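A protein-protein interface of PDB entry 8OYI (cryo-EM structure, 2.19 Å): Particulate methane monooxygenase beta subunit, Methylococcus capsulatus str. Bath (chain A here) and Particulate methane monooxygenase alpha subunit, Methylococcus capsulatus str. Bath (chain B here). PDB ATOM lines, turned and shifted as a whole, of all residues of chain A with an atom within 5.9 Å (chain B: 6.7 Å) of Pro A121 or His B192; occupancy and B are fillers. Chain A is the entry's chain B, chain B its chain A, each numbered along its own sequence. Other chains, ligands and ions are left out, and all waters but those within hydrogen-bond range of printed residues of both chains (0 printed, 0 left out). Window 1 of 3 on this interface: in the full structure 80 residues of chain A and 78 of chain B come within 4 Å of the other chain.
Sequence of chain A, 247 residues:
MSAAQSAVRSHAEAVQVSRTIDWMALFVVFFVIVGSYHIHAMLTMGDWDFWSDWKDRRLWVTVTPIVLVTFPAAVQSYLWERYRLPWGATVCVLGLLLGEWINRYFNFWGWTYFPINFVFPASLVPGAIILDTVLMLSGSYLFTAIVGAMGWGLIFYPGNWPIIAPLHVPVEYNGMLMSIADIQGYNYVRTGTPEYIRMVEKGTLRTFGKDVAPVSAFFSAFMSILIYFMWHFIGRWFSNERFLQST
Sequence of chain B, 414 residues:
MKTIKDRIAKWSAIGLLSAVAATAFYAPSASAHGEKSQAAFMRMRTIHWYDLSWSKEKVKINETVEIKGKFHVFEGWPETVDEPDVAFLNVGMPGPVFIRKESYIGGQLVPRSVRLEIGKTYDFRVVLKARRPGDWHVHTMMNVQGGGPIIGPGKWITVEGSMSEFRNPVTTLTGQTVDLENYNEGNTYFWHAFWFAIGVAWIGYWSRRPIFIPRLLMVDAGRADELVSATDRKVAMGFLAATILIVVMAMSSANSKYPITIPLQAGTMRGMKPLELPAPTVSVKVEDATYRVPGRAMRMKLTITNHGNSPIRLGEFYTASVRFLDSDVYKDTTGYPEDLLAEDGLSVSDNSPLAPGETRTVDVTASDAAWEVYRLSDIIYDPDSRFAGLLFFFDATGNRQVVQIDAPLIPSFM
A ring nitrogen (ND1) of His B192 sits at hydrogen-bond distance from the indole nitrogen of Trp A101 (3.1 Å). A ring nitrogen (NE2) of His B192 lies within hydrogen-bond range of the backbone carbonyl oxygen of Pro A121 (2.6 Å).
The side-chain amide oxygen of Asn A160 sits at hydrogen-bond distance from the backbone NH of Ser A123 (2.5 Å). NZ of Lys A55 is in hydrogen-bond range of O of Phe A120 (3.3 Å). OD1 of Asn B187 lies close to NE1 of Trp B191. OD1 of Asp A49 sits at hydrogen-bond distance from N of Ala A122.
His B192 touches Leu A97. CE1 of Tyr B189 touches CZ3 of Trp A101, 3.5 Å away. CG2 of Thr B188 touches CB of Phe A120 (3.5 Å). His B192 touches Ala A122. His B192 touches Ser A123 (CE1 to N, 3.9 Å). OG of Ser A123 touches CD1 of Trp B195, 3.5 Å away. ND2 of Asn B187 touches CA of Ile A163, at 3.6 Å. Thr B188 touches Ile A163 (OG1 to CG2, 3.5 Å). Ile A163 touches Trp B191 (CG1 to CB, 3.6 Å).
Pro A121 touches just one residue of chain B: His B192. Of chain A, only Leu A97 (3.97 Å), Trp A101 (3.1 Å), Pro A121 (2.6 Å), Ala A122 (3.3 Å) and Ser A123 (3.9 Å) come within 4 Å of His B192. Of the printed residues of chain B, Phe A120 touches Thr B188. Printed residues of chain A within 4 Å of Asn B187: Ile A163. Printed residues of chain A within 4 Å of Tyr B189: Trp A101. Of the printed residues of chain A, Trp B195 touches Ser A123 (3.5 Å). Printed residues of chain B within 4 Å of Leu A97: His B192.
Of the 11 printed residues of chain B, 6 touch a printed residue of chain A. Among the printed residues, no Asp or Glu carboxylate lies within 4 Å of a Lys or Arg side-chain nitrogen of the other chain.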
ATOM      1  N   ASP A  49      -8.938   5.953  18.242  1.00  0.00           N
ATOM      2  CA  ASP A  49      -9.774   6.924  17.551  1.00  0.00           C
ATOM      3  C   ASP A  49     -10.831   7.548  18.452  1.00  0.00           C
ATOM      4  O   ASP A  49     -11.321   8.637  18.140  1.00  0.00           O
ATOM      5  CB  ASP A  49     -10.452   6.269  16.347  1.00  0.00           C
ATOM      6  CG  ASP A  49     -11.039   7.284  15.388  1.00  0.00           C
ATOM      7  OD1 ASP A  49     -10.270   8.104  14.845  1.00  0.00           O
ATOM      8  OD2 ASP A  49     -12.271   7.267  15.185  1.00  0.00           O
ATOM      9  N   LYS A  55      -4.812   9.503  21.593  1.00  0.00           N
ATOM     10  CA  LYS A  55      -4.090   9.926  20.387  1.00  0.00           C
ATOM     11  C   LYS A  55      -2.643  10.270  20.745  1.00  0.00           C
ATOM     12  O   LYS A  55      -2.264  11.433  20.908  1.00  0.00           O
ATOM     13  CB  LYS A  55      -4.779  11.112  19.724  1.00  0.00           C
ATOM     14  CG  LYS A  55      -6.283  11.003  19.643  1.00  0.00           C
ATOM     15  CD  LYS A  55      -6.744  10.624  18.254  1.00  0.00           C
ATOM     16  CE  LYS A  55      -8.218  10.915  18.063  1.00  0.00           C
ATOM     17  NZ  LYS A  55      -9.051  10.061  18.946  1.00  0.00           N
ATOM     18  N   LEU A  97     -15.125   8.196   7.906  1.00  0.00           N
ATOM     19  CA  LEU A  97     -15.222   9.452   8.643  1.00  0.00           C
ATOM     20  C   LEU A  97     -16.670   9.836   8.892  1.00  0.00           C
ATOM     21  O   LEU A  97     -17.008  10.332   9.970  1.00  0.00           O
ATOM     22  CB  LEU A  97     -14.495  10.561   7.885  1.00  0.00           C
ATOM     23  CG  LEU A  97     -12.978  10.601   8.065  1.00  0.00           C
ATOM     24  CD1 LEU A  97     -12.337  11.461   6.995  1.00  0.00           C
ATOM     25  CD2 LEU A  97     -12.622  11.114   9.447  1.00  0.00           C
ATOM     26  N   GLU A 100     -18.044   7.503  11.626  1.00  0.00           N
ATOM     27  CA  GLU A 100     -17.419   7.834  12.897  1.00  0.00           C
ATOM     28  C   GLU A 100     -17.969   9.139  13.453  1.00  0.00           C
ATOM     29  O   GLU A 100     -18.302   9.224  14.635  1.00  0.00           O
ATOM     30  CB  GLU A 100     -15.903   7.912  12.726  1.00  0.00           C
ATOM     31  CG  GLU A 100     -15.211   6.561  12.760  1.00  0.00           C
ATOM     32  CD  GLU A 100     -13.742   6.646  12.409  1.00  0.00           C
ATOM     33  OE1 GLU A 100     -13.365   7.548  11.635  1.00  0.00           O
ATOM     34  OE2 GLU A 100     -12.963   5.800  12.896  1.00  0.00           O
ATOM     35  N   TRP A 101     -18.088  10.168  12.609  1.00  0.00           N
ATOM     36  CA  TRP A 101     -18.588  11.457  13.073  1.00  0.00           C
ATOM     37  C   TRP A 101     -20.050  11.382  13.476  1.00  0.00           C
ATOM     38  O   TRP A 101     -20.450  12.002  14.467  1.00  0.00           O
ATOM     39  CB  TRP A 101     -18.391  12.524  11.996  1.00  0.00           C
ATOM     40  CG  TRP A 101     -17.145  13.324  12.181  1.00  0.00           C
ATOM     41  CD1 TRP A 101     -16.051  13.336  11.368  1.00  0.00           C
ATOM     42  CD2 TRP A 101     -16.858  14.225  13.253  1.00  0.00           C
ATOM     43  NE1 TRP A 101     -15.102  14.192  11.865  1.00  0.00           N
ATOM     44  CE2 TRP A 101     -15.573  14.753  13.023  1.00  0.00           C
ATOM     45  CE3 TRP A 101     -17.563  14.644  14.387  1.00  0.00           C
ATOM     46  CZ2 TRP A 101     -14.978  15.672  13.882  1.00  0.00           C
ATOM     47  CZ3 TRP A 101     -16.971  15.556  15.237  1.00  0.00           C
ATOM     48  CH2 TRP A 101     -15.690  16.059  14.981  1.00  0.00           C
ATOM     49  N   ARG A 104     -19.998   9.773  16.850  1.00  0.00           N
ATOM     50  CA  ARG A 104     -19.440  10.678  17.849  1.00  0.00           C
ATOM     51  C   ARG A 104     -20.456  11.735  18.253  1.00  0.00           C
ATOM     52  O   ARG A 104     -20.638  12.009  19.446  1.00  0.00           O
ATOM     53  CB  ARG A 104     -18.181  11.370  17.318  1.00  0.00           C
ATOM     54  CG  ARG A 104     -16.994  10.479  17.002  1.00  0.00           C
ATOM     55  CD  ARG A 104     -16.842   9.323  17.953  1.00  0.00           C
ATOM     56  NE  ARG A 104     -16.246   8.176  17.281  1.00  0.00           N
ATOM     57  CZ  ARG A 104     -14.948   8.026  17.063  1.00  0.00           C
ATOM     58  NH1 ARG A 104     -14.070   8.937  17.459  1.00  0.00           N
ATOM     59  NH2 ARG A 104     -14.516   6.944  16.427  1.00  0.00           N
ATOM     60  N   VAL A 119     -13.882  13.452  21.956  1.00  0.00           N
ATOM     61  CA  VAL A 119     -14.185  12.208  21.251  1.00  0.00           C
ATOM     62  C   VAL A 119     -14.111  12.371  19.730  1.00  0.00           C
ATOM     63  O   VAL A 119     -14.695  11.576  19.001  1.00  0.00           O
ATOM     64  CB  VAL A 119     -15.548  11.644  21.678  1.00  0.00           C
ATOM     65  CG1 VAL A 119     -15.519  11.258  23.142  1.00  0.00           C
ATOM     66  CG2 VAL A 119     -16.656  12.646  21.400  1.00  0.00           C
ATOM     67  N   PHE A 120     -13.394  13.377  19.235  1.00  0.00           N
ATOM     68  CA  PHE A 120     -13.280  13.557  17.795  1.00  0.00           C
ATOM     69  C   PHE A 120     -12.482  12.413  17.162  1.00  0.00           C
ATOM     70  O   PHE A 120     -11.586  11.847  17.789  1.00  0.00           O
ATOM     71  CB  PHE A 120     -12.607  14.887  17.478  1.00  0.00           C
ATOM     72  CG  PHE A 120     -11.206  14.998  18.003  1.00  0.00           C
ATOM     73  CD1 PHE A 120     -10.971  15.466  19.283  1.00  0.00           C
ATOM     74  CD2 PHE A 120     -10.125  14.634  17.217  1.00  0.00           C
ATOM     75  CE1 PHE A 120      -9.686  15.562  19.770  1.00  0.00           C
ATOM     76  CE2 PHE A 120      -8.839  14.731  17.702  1.00  0.00           C
ATOM     77  CZ  PHE A 120      -8.620  15.196  18.979  1.00  0.00           C
ATOM     78  N   PRO A 121     -12.788  12.060  15.919  1.00  0.00           N
ATOM     79  CA  PRO A 121     -12.009  11.043  15.205  1.00  0.00           C
ATOM     80  C   PRO A 121     -10.768  11.653  14.557  1.00  0.00           C
ATOM     81  O   PRO A 121     -10.580  12.867  14.524  1.00  0.00           O
ATOM     82  CB  PRO A 121     -12.993  10.532  14.153  1.00  0.00           C
ATOM     83  CG  PRO A 121     -13.865  11.700  13.880  1.00  0.00           C
ATOM     84  CD  PRO A 121     -13.988  12.463  15.167  1.00  0.00           C
ATOM     85  N   ALA A 122      -9.912  10.775  14.042  1.00  0.00           N
ATOM     86  CA  ALA A 122      -8.704  11.178  13.335  1.00  0.00           C
ATOM     87  C   ALA A 122      -9.016  11.528  11.885  1.00  0.00           C
ATOM     88  O   ALA A 122     -10.042  11.127  11.332  1.00  0.00           O
ATOM     89  CB  ALA A 122      -7.655  10.066  13.384  1.00  0.00           C
ATOM     90  N   SER A 123      -8.112  12.292  11.272  1.00  0.00           N
ATOM     91  CA  SER A 123      -8.239  12.693   9.877  1.00  0.00           C
ATOM     92  C   SER A 123      -7.440  11.743   8.986  1.00  0.00           C
ATOM     93  O   SER A 123      -6.313  11.371   9.324  1.00  0.00           O
ATOM     94  CB  SER A 123      -7.757  14.132   9.689  1.00  0.00           C
ATOM     95  OG  SER A 123      -7.923  14.558   8.349  1.00  0.00           O
ATOM     96  N   ASN A 160      -2.929  15.098  11.185  1.00  0.00           N
ATOM     97  CA  ASN A 160      -3.721  15.284  12.391  1.00  0.00           C
ATOM     98  C   ASN A 160      -3.099  16.255  13.382  1.00  0.00           C
ATOM     99  O   ASN A 160      -3.752  16.615  14.364  1.00  0.00           O
ATOM    100  CB  ASN A 160      -3.955  13.941  13.086  1.00  0.00           C
ATOM    101  CG  ASN A 160      -4.947  13.069  12.350  1.00  0.00           C
ATOM    102  OD1 ASN A 160      -6.157  13.205  12.524  1.00  0.00           O
ATOM    103  ND2 ASN A 160      -4.440  12.163  11.525  1.00  0.00           N
ATOM    104  N   ILE A 163      -5.010  19.430  14.491  1.00  0.00           N
ATOM    105  CA  ILE A 163      -6.161  19.191  15.356  1.00  0.00           C
ATOM    106  C   ILE A 163      -5.723  18.939  16.794  1.00  0.00           C
ATOM    107  O   ILE A 163      -6.285  19.507  17.736  1.00  0.00           O
ATOM    108  CB  ILE A 163      -7.003  18.022  14.811  1.00  0.00           C
ATOM    109  CG1 ILE A 163      -7.513  18.341  13.405  1.00  0.00           C
ATOM    110  CG2 ILE A 163      -8.162  17.719  15.740  1.00  0.00           C
ATOM    111  CD1 ILE A 163      -7.744  17.118  12.553  1.00  0.00           C
ATOM    112  N   ASN B 187     -11.599  24.381  16.034  1.00  0.00           N
ATOM    113  CA  ASN B 187     -10.474  23.973  15.201  1.00  0.00           C
ATOM    114  C   ASN B 187     -10.655  22.549  14.686  1.00  0.00           C
ATOM    115  O   ASN B 187     -10.404  22.267  13.505  1.00  0.00           O
ATOM    116  CB  ASN B 187      -9.175  24.104  15.996  1.00  0.00           C
ATOM    117  CG  ASN B 187      -7.965  23.640  15.220  1.00  0.00           C
ATOM    118  OD1 ASN B 187      -7.614  24.219  14.196  1.00  0.00           O
ATOM    119  ND2 ASN B 187      -7.309  22.595  15.714  1.00  0.00           N
ATOM    120  N   THR B 188     -11.098  21.640  15.559  1.00  0.00           N
ATOM    121  CA  THR B 188     -11.340  20.263  15.142  1.00  0.00           C
ATOM    122  C   THR B 188     -12.409  20.196  14.057  1.00  0.00           C
ATOM    123  O   THR B 188     -12.213  19.541  13.021  1.00  0.00           O
ATOM    124  CB  THR B 188     -11.759  19.416  16.343  1.00  0.00           C
ATOM    125  OG1 THR B 188     -10.721  19.437  17.330  1.00  0.00           O
ATOM    126  CG2 THR B 188     -12.019  17.988  15.916  1.00  0.00           C
ATOM    127  N   TYR B 189     -13.535  20.876  14.276  1.00  0.00           N
ATOM    128  CA  TYR B 189     -14.601  20.901  13.283  1.00  0.00           C
ATOM    129  C   TYR B 189     -14.103  21.466  11.962  1.00  0.00           C
ATOM    130  O   TYR B 189     -14.385  20.915  10.893  1.00  0.00           O
ATOM    131  CB  TYR B 189     -15.785  21.721  13.796  1.00  0.00           C
ATOM    132  CG  TYR B 189     -16.744  20.954  14.668  1.00  0.00           C
ATOM    133  CD1 TYR B 189     -17.018  19.614  14.425  1.00  0.00           C
ATOM    134  CD2 TYR B 189     -17.393  21.570  15.728  1.00  0.00           C
ATOM    135  CE1 TYR B 189     -17.900  18.911  15.213  1.00  0.00           C
ATOM    136  CE2 TYR B 189     -18.277  20.874  16.524  1.00  0.00           C
ATOM    137  CZ  TYR B 189     -18.528  19.547  16.263  1.00  0.00           C
ATOM    138  OH  TYR B 189     -19.410  18.853  17.055  1.00  0.00           O
ATOM    139  N   PHE B 190     -13.348  22.564  12.019  1.00  0.00           N
ATOM    140  CA  PHE B 190     -12.869  23.210  10.803  1.00  0.00           C
ATOM    141  C   PHE B 190     -11.979  22.276  10.002  1.00  0.00           C
ATOM    142  O   PHE B 190     -12.158  22.113   8.791  1.00  0.00           O
ATOM    143  CB  PHE B 190     -12.116  24.494  11.151  1.00  0.00           C
ATOM    144  CG  PHE B 190     -11.278  25.021  10.022  1.00  0.00           C
ATOM    145  CD1 PHE B 190     -11.849  25.785   9.018  1.00  0.00           C
ATOM    146  CD2 PHE B 190      -9.919  24.752   9.959  1.00  0.00           C
ATOM    147  CE1 PHE B 190     -11.087  26.268   7.976  1.00  0.00           C
ATOM    148  CE2 PHE B 190      -9.152  25.231   8.917  1.00  0.00           C
ATOM    149  CZ  PHE B 190      -9.736  25.991   7.925  1.00  0.00           C
ATOM    150  N   TRP B 191     -10.995  21.659  10.658  1.00  0.00           N
ATOM    151  CA  TRP B 191     -10.061  20.813   9.920  1.00  0.00           C
ATOM    152  C   TRP B 191     -10.750  19.576   9.360  1.00  0.00           C
ATOM    153  O   TRP B 191     -10.502  19.186   8.207  1.00  0.00           O
ATOM    154  CB  TRP B 191      -8.883  20.428  10.812  1.00  0.00           C
ATOM    155  CG  TRP B 191      -7.848  21.502  10.864  1.00  0.00           C
ATOM    156  CD1 TRP B 191      -7.458  22.213  11.957  1.00  0.00           C
ATOM    157  CD2 TRP B 191      -7.092  22.014   9.760  1.00  0.00           C
ATOM    158  NE1 TRP B 191      -6.495  23.125  11.609  1.00  0.00           N
ATOM    159  CE2 TRP B 191      -6.252  23.024  10.266  1.00  0.00           C
ATOM    160  CE3 TRP B 191      -7.037  21.710   8.398  1.00  0.00           C
ATOM    161  CZ2 TRP B 191      -5.370  23.730   9.456  1.00  0.00           C
ATOM    162  CZ3 TRP B 191      -6.160  22.414   7.597  1.00  0.00           C
ATOM    163  CH2 TRP B 191      -5.340  23.414   8.128  1.00  0.00           C
ATOM    164  N   HIS B 192     -11.632  18.954  10.150  1.00  0.00           N
ATOM    165  CA  HIS B 192     -12.333  17.778   9.648  1.00  0.00           C
ATOM    166  C   HIS B 192     -13.233  18.130   8.471  1.00  0.00           C
ATOM    167  O   HIS B 192     -13.256  17.409   7.466  1.00  0.00           O
ATOM    168  CB  HIS B 192     -13.131  17.121  10.771  1.00  0.00           C
ATOM    169  CG  HIS B 192     -12.370  16.060  11.501  1.00  0.00           C
ATOM    170  ND1 HIS B 192     -12.222  14.781  11.009  1.00  0.00           N
ATOM    171  CD2 HIS B 192     -11.696  16.093  12.674  1.00  0.00           C
ATOM    172  CE1 HIS B 192     -11.497  14.069  11.855  1.00  0.00           C
ATOM    173  NE2 HIS B 192     -11.166  14.841  12.873  1.00  0.00           N
ATOM    174  N   ALA B 193     -13.958  19.251   8.562  1.00  0.00           N
ATOM    175  CA  ALA B 193     -14.803  19.681   7.457  1.00  0.00           C
ATOM    176  C   ALA B 193     -13.974  20.013   6.225  1.00  0.00           C
ATOM    177  O   ALA B 193     -14.379  19.701   5.103  1.00  0.00           O
ATOM    178  CB  ALA B 193     -15.647  20.881   7.877  1.00  0.00           C
ATOM    179  N   PHE B 194     -12.812  20.641   6.413  1.00  0.00           N
ATOM    180  CA  PHE B 194     -11.953  20.985   5.285  1.00  0.00           C
ATOM    181  C   PHE B 194     -11.488  19.738   4.545  1.00  0.00           C
ATOM    182  O   PHE B 194     -11.573  19.660   3.312  1.00  0.00           O
ATOM    183  CB  PHE B 194     -10.761  21.806   5.784  1.00  0.00           C
ATOM    184  CG  PHE B 194      -9.706  22.050   4.746  1.00  0.00           C
ATOM    185  CD1 PHE B 194      -9.782  23.151   3.909  1.00  0.00           C
ATOM    186  CD2 PHE B 194      -8.619  21.195   4.620  1.00  0.00           C
ATOM    187  CE1 PHE B 194      -8.809  23.385   2.957  1.00  0.00           C
ATOM    188  CE2 PHE B 194      -7.644  21.424   3.671  1.00  0.00           C
ATOM    189  CZ  PHE B 194      -7.738  22.521   2.839  1.00  0.00           C
ATOM    190  N   TRP B 195     -10.999  18.740   5.284  1.00  0.00           N
ATOM    191  CA  TRP B 195     -10.500  17.544   4.614  1.00  0.00           C
ATOM    192  C   TRP B 195     -11.636  16.732   4.001  1.00  0.00           C
ATOM    193  O   TRP B 195     -11.496  16.178   2.902  1.00  0.00           O
ATOM    194  CB  TRP B 195      -9.673  16.706   5.587  1.00  0.00           C
ATOM    195  CG  TRP B 195      -8.310  17.286   5.797  1.00  0.00           C
ATOM    196  CD1 TRP B 195      -7.782  17.736   6.970  1.00  0.00           C
ATOM    197  CD2 TRP B 195      -7.313  17.517   4.794  1.00  0.00           C
ATOM    198  NE1 TRP B 195      -6.514  18.214   6.764  1.00  0.00           N
ATOM    199  CE2 TRP B 195      -6.201  18.092   5.437  1.00  0.00           C
ATOM    200  CE3 TRP B 195      -7.247  17.282   3.415  1.00  0.00           C
ATOM    201  CZ2 TRP B 195      -5.039  18.438   4.752  1.00  0.00           C
ATOM    202  CZ3 TRP B 195      -6.095  17.625   2.738  1.00  0.00           C
ATOM    203  CH2 TRP B 195      -5.006  18.198   3.406  1.00  0.00           C
ATOM    204  N   PHE B 196     -12.786  16.672   4.683  1.00  0.00           N
ATOM    205  CA  PHE B 196     -13.948  16.012   4.102  1.00  0.00           C
ATOM    206  C   PHE B 196     -14.377  16.702   2.815  1.00  0.00           C
ATOM    207  O   PHE B 196     -14.747  16.037   1.840  1.00  0.00           O
ATOM    208  CB  PHE B 196     -15.092  15.988   5.112  1.00  0.00           C
ATOM    209  CG  PHE B 196     -16.077  14.883   4.887  1.00  0.00           C
ATOM    210  CD1 PHE B 196     -17.144  15.051   4.021  1.00  0.00           C
ATOM    211  CD2 PHE B 196     -15.939  13.671   5.545  1.00  0.00           C
ATOM    212  CE1 PHE B 196     -18.052  14.033   3.812  1.00  0.00           C
ATOM    213  CE2 PHE B 196     -16.846  12.649   5.339  1.00  0.00           C
ATOM    214  CZ  PHE B 196     -17.902  12.830   4.472  1.00  0.00           C
ATOM    215  N   ALA B 197     -14.334  18.036   2.793  1.00  0.00           N
ATOM    216  CA  ALA B 197     -14.681  18.780   1.590  1.00  0.00           C
ATOM    217  C   ALA B 197     -13.699  18.497   0.465  1.00  0.00           C
ATOM    218  O   ALA B 197     -14.096  18.396  -0.697  1.00  0.00           O
ATOM    219  CB  ALA B 197     -14.734  20.276   1.895  1.00  0.00           C
